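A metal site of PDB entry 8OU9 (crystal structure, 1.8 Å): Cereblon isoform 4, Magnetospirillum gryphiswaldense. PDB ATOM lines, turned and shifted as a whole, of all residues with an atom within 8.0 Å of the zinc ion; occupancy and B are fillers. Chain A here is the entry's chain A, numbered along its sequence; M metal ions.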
ATOM      1  N   ARG A   6      22.751   1.939 -12.006  1.00  0.00           N
ATOM      2  CA  ARG A   6      23.023   1.259 -13.246  1.00  0.00           C
ATOM      3  C   ARG A   6      23.867   0.027 -12.964  1.00  0.00           C
ATOM      4  O   ARG A   6      24.559  -0.008 -11.965  1.00  0.00           O
ATOM      5  CB  ARG A   6      23.748   2.223 -14.236  1.00  0.00           C
ATOM      6  CG  ARG A   6      22.818   3.271 -14.837  1.00  0.00           C
ATOM      7  CD  ARG A   6      23.528   4.188 -15.872  1.00  0.00           C
ATOM      8  NE  ARG A   6      22.536   5.199 -16.291  1.00  0.00           N
ATOM      9  CZ  ARG A   6      21.532   4.980 -17.108  1.00  0.00           C
ATOM     10  NH1 ARG A   6      21.381   3.788 -17.647  1.00  0.00           N
ATOM     11  NH2 ARG A   6      20.661   5.942 -17.262  1.00  0.00           N
ATOM     12  N   CYS A   7      23.829  -0.923 -13.919  1.00  0.00           N
ATOM     13  CA  CYS A   7      24.756  -2.041 -13.893  1.00  0.00           C
ATOM     14  C   CYS A   7      26.190  -1.519 -13.966  1.00  0.00           C
ATOM     15  O   CYS A   7      26.503  -0.837 -14.904  1.00  0.00           O
ATOM     16  CB  CYS A   7      24.441  -3.092 -14.954  1.00  0.00           C
ATOM     17  SG  CYS A   7      25.664  -4.462 -15.044  1.00  0.00           S
ATOM     18  N   ARG A   8      27.069  -1.928 -13.035  1.00  0.00           N
ATOM     19  CA  ARG A   8      28.441  -1.424 -13.041  1.00  0.00           C
ATOM     20  C   ARG A   8      29.222  -1.930 -14.258  1.00  0.00           C
ATOM     21  O   ARG A   8      30.197  -1.266 -14.620  1.00  0.00           O
ATOM     22  CB  ARG A   8      29.231  -1.781 -11.767  1.00  0.00           C
ATOM     23  N   GLN A   9      28.852  -3.078 -14.803  1.00  0.00           N
ATOM     24  CA  GLN A   9      29.555  -3.673 -15.945  1.00  0.00           C
ATOM     25  C   GLN A   9      29.171  -3.021 -17.276  1.00  0.00           C
ATOM     26  O   GLN A   9      29.982  -2.960 -18.154  1.00  0.00           O
ATOM     27  CB  GLN A   9      29.281  -5.176 -15.944  1.00  0.00           C
ATOM     28  CG  GLN A   9      30.073  -5.986 -16.970  1.00  0.00           C
ATOM     29  CD  GLN A   9      31.550  -6.099 -16.631  1.00  0.00           C
ATOM     30  OE1 GLN A   9      32.002  -5.728 -15.538  1.00  0.00           O
ATOM     31  NE2 GLN A   9      32.320  -6.633 -17.567  1.00  0.00           N
ATOM     32  N   CYS A  10      27.947  -2.543 -17.479  1.00  0.00           N
ATOM     33  CA  CYS A  10      27.558  -2.174 -18.830  1.00  0.00           C
ATOM     34  C   CYS A  10      26.728  -0.905 -18.848  1.00  0.00           C
ATOM     35  O   CYS A  10      26.426  -0.409 -19.901  1.00  0.00           O
ATOM     36  CB  CYS A  10      26.869  -3.389 -19.414  1.00  0.00           C
ATOM     37  SG  CYS A  10      25.160  -3.579 -18.796  1.00  0.00           S
ATOM     38  N   GLY A  11      26.161  -0.464 -17.703  1.00  0.00           N
ATOM     39  CA  GLY A  11      25.387   0.750 -17.748  1.00  0.00           C
ATOM     40  C   GLY A  11      23.891   0.600 -17.855  1.00  0.00           C
ATOM     41  O   GLY A  11      23.170   1.618 -17.798  1.00  0.00           O
ATOM     42  N   GLN A  12      23.388  -0.609 -17.986  1.00  0.00           N
ATOM     43  CA  GLN A  12      21.951  -0.853 -18.020  1.00  0.00           C
ATOM     44  C   GLN A  12      21.273  -0.157 -16.832  1.00  0.00           C
ATOM     45  O   GLN A  12      21.766  -0.260 -15.712  1.00  0.00           O
ATOM     46  CB  GLN A  12      21.664  -2.353 -17.911  1.00  0.00           C
ATOM     47  CG  GLN A  12      20.216  -2.758 -17.763  1.00  0.00           C
ATOM     48  CD  GLN A  12      19.537  -2.868 -19.095  1.00  0.00           C
ATOM     49  OE1 GLN A  12      19.677  -2.043 -19.984  1.00  0.00           O
ATOM     50  NE2 GLN A  12      18.853  -3.995 -19.273  1.00  0.00           N
ATOM     51  N   THR A  13      20.162   0.543 -17.088  1.00  0.00           N
ATOM     52  CA  THR A  13      19.330   1.122 -16.045  1.00  0.00           C
ATOM     53  C   THR A  13      18.704   0.034 -15.178  1.00  0.00           C
ATOM     54  O   THR A  13      18.058  -0.879 -15.743  1.00  0.00           O
ATOM     55  CB  THR A  13      18.176   1.891 -16.721  1.00  0.00           C
ATOM     56  OG1 THR A  13      18.727   2.658 -17.790  1.00  0.00           O
ATOM     57  CG2 THR A  13      17.394   2.724 -15.737  1.00  0.00           C
ATOM     58  N   ILE A  14      18.855   0.127 -13.841  1.00  0.00           N
ATOM     59  CA  ILE A  14      18.397  -0.933 -12.948  1.00  0.00           C
ATOM     60  C   ILE A  14      17.398  -0.404 -11.902  1.00  0.00           C
ATOM     61  O   ILE A  14      16.325  -0.973 -11.728  1.00  0.00           O
ATOM     62  CB  ILE A  14      19.541  -1.665 -12.221  1.00  0.00           C
ATOM     63  CG1 ILE A  14      20.531  -2.304 -13.214  1.00  0.00           C
ATOM     64  CG2 ILE A  14      18.927  -2.745 -11.326  1.00  0.00           C
ATOM     65  CD1 ILE A  14      19.954  -3.387 -14.118  1.00  0.00           C
ATOM     66  N   GLY A  49      15.297  -3.687 -16.039  1.00  0.00           N
ATOM     67  CA  GLY A  49      16.466  -4.010 -16.826  1.00  0.00           C
ATOM     68  C   GLY A  49      17.120  -5.351 -16.484  1.00  0.00           C
ATOM     69  O   GLY A  49      18.256  -5.582 -16.948  1.00  0.00           O
ATOM     70  N   LEU A  72      19.730 -11.530 -13.262  1.00  0.00           N
ATOM     71  CA  LEU A  72      20.847 -11.052 -14.050  1.00  0.00           C
ATOM     72  C   LEU A  72      20.548  -9.699 -14.648  1.00  0.00           C
ATOM     73  O   LEU A  72      19.395  -9.324 -14.893  1.00  0.00           O
ATOM     74  CB  LEU A  72      21.087 -12.050 -15.197  1.00  0.00           C
ATOM     75  CG  LEU A  72      21.300 -13.513 -14.775  1.00  0.00           C
ATOM     76  CD1 LEU A  72      21.600 -14.349 -16.001  1.00  0.00           C
ATOM     77  CD2 LEU A  72      22.402 -13.679 -13.777  1.00  0.00           C
ATOM     78  N   CYS A  73      21.643  -8.966 -14.983  1.00  0.00           N
ATOM     79  CA  CYS A  73      21.476  -7.799 -15.770  1.00  0.00           C
ATOM     80  C   CYS A  73      20.882  -8.323 -17.081  1.00  0.00           C
ATOM     81  O   CYS A  73      21.524  -9.205 -17.677  1.00  0.00           O
ATOM     82  CB  CYS A  73      22.849  -7.136 -15.998  1.00  0.00           C
ATOM     83  SG  CYS A  73      22.771  -5.733 -17.153  1.00  0.00           S
ATOM     84  N   GLY A  74      19.839  -7.697 -17.562  1.00  0.00           N
ATOM     85  CA  GLY A  74      19.196  -8.143 -18.812  1.00  0.00           C
ATOM     86  C   GLY A  74      20.069  -7.858 -20.029  1.00  0.00           C
ATOM     87  O   GLY A  74      19.904  -8.460 -21.062  1.00  0.00           O
ATOM     88  N   GLN A  75      21.063  -6.941 -19.909  1.00  0.00           N
ATOM     89  CA  GLN A  75      21.849  -6.532 -21.047  1.00  0.00           C
ATOM     90  C   GLN A  75      23.099  -7.410 -21.092  1.00  0.00           C
ATOM     91  O   GLN A  75      23.412  -8.123 -22.043  1.00  0.00           O
ATOM     92  CB  GLN A  75      22.155  -5.046 -20.927  1.00  0.00           C
ATOM     93  CG  GLN A  75      23.015  -4.455 -22.002  1.00  0.00           C
ATOM     94  CD  GLN A  75      22.873  -2.964 -22.076  1.00  0.00           C
ATOM     95  OE1 GLN A  75      22.116  -2.465 -22.903  1.00  0.00           O
ATOM     96  NE2 GLN A  75      23.655  -2.239 -21.292  1.00  0.00           N
ATOM     97  N   CYS A  76      23.834  -7.464 -19.992  1.00  0.00           N
ATOM     98  CA  CYS A  76      25.153  -8.058 -20.035  1.00  0.00           C
ATOM     99  C   CYS A  76      25.204  -9.449 -19.420  1.00  0.00           C
ATOM    100  O   CYS A  76      26.208 -10.161 -19.536  1.00  0.00           O
ATOM    101  CB  CYS A  76      26.283  -7.191 -19.478  1.00  0.00           C
ATOM    102  SG  CYS A  76      26.317  -7.072 -17.635  1.00  0.00           S
ATOM    103  N   GLY A  77      24.203  -9.843 -18.632  1.00  0.00           N
ATOM    104  CA  GLY A  77      24.160 -11.139 -18.012  1.00  0.00           C
ATOM    105  C   GLY A  77      24.861 -11.230 -16.648  1.00  0.00           C
ATOM    106  O   GLY A  77      24.953 -12.307 -16.125  1.00  0.00           O
ATOM    107  N   SER A  78      25.434 -10.168 -16.123  1.00  0.00           N
ATOM    108  CA  SER A  78      26.080 -10.152 -14.826  1.00  0.00           C
ATOM    109  C   SER A  78      25.052 -10.469 -13.743  1.00  0.00           C
ATOM    110  O   SER A  78      23.905 -10.002 -13.819  1.00  0.00           O
ATOM    111  CB  SER A  78      26.729  -8.794 -14.594  1.00  0.00           C
ATOM    112  OG  SER A  78      27.145  -8.583 -13.232  1.00  0.00           O
ATOM    113  N   HIS A  79      25.465 -11.254 -12.729  1.00  0.00           N
ATOM    114  CA  HIS A  79      24.578 -11.530 -11.611  1.00  0.00           C
ATOM    115  C   HIS A  79      24.431 -10.331 -10.722  1.00  0.00           C
ATOM    116  O   HIS A  79      25.412  -9.900 -10.103  1.00  0.00           O
ATOM    117  CB  HIS A  79      25.135 -12.738 -10.847  1.00  0.00           C
ATOM    118  CG  HIS A  79      24.252 -13.092  -9.721  1.00  0.00           C
ATOM    119  ND1 HIS A  79      24.758 -13.597  -8.533  1.00  0.00           N
ATOM    120  CD2 HIS A  79      22.909 -12.932  -9.531  1.00  0.00           C
ATOM    121  CE1 HIS A  79      23.734 -13.840  -7.704  1.00  0.00           C
ATOM    122  NE2 HIS A  79      22.616 -13.461  -8.266  1.00  0.00           N
ATOM    123  N   LEU A  80      23.259  -9.710 -10.673  1.00  0.00           N
ATOM    124  CA  LEU A  80      23.046  -8.531  -9.889  1.00  0.00           C
ATOM    125  C   LEU A  80      22.286  -8.727  -8.577  1.00  0.00           C
ATOM    126  O   LEU A  80      22.334  -7.821  -7.746  1.00  0.00           O
ATOM    127  CB  LEU A  80      22.277  -7.475 -10.713  1.00  0.00           C
ATOM    128  CG  LEU A  80      23.001  -6.894 -11.933  1.00  0.00           C
ATOM    129  CD1 LEU A  80      22.253  -5.701 -12.575  1.00  0.00           C
ATOM    130  CD2 LEU A  80      24.400  -6.486 -11.625  1.00  0.00           C
ATOM    131  N   ARG A 100      27.697  -4.261  -7.243  1.00  0.00           N
ATOM    132  CA  ARG A 100      27.557  -4.598  -8.660  1.00  0.00           C
ATOM    133  C   ARG A 100      26.815  -3.488  -9.411  1.00  0.00           C
ATOM    134  O   ARG A 100      26.534  -3.659 -10.586  1.00  0.00           O
ATOM    135  CB  ARG A 100      26.939  -5.950  -8.822  1.00  0.00           C
ATOM    136  CG  ARG A 100      27.908  -6.976  -8.212  1.00  0.00           C
ATOM    137  CD  ARG A 100      27.650  -8.390  -8.612  1.00  0.00           C
ATOM    138  NE  ARG A 100      28.517  -9.299  -7.843  1.00  0.00           N
ATOM    139  CZ  ARG A 100      28.369 -10.623  -7.794  1.00  0.00           C
ATOM    140  NH1 ARG A 100      27.430 -11.243  -8.496  1.00  0.00           N
ATOM    141  NH2 ARG A 100      29.161 -11.353  -7.022  1.00  0.00           N
HETATM  142 ZN    ZN M   1      25.078  -5.255 -17.123  1.00  0.00          ZN
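The side-chain sulfur (SG) of Cys 7 sits close to the backbone NH (N) of Gln 9.
The side-chain sulfur of Cys 76 sits close to the backbone NH of Ser 78.
The backbone carbonyl oxygen of Gln 12 lies within hydrogen-bond range of the backbone NH of Cys 7 (2.8 Å).
The side-chain sulfur (SG) of Cys 10 sits close to the side-chain amide nitrogen (NE2) of Gln 75 (3.2 Å).
SG of Cys 10 sits close to N of Gln 12 (3.6 Å).
The backbone NH (N) of Gln 75 sits close to the side-chain sulfur (SG) of Cys 73.
The backbone NH (N) of Cys 73 lies within hydrogen-bond range of the backbone carbonyl oxygen (O) of Ser 78, at 2.7 Å.
The zinc ion is bound by the side-chain sulfur of Cys 76, the side-chain sulfur of Cys 7, the side-chain sulfur of Cys 73 and the side-chain sulfur of Cys 10.
Of the 20 residues printed, 4 come within 4 Å of the zinc ion.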
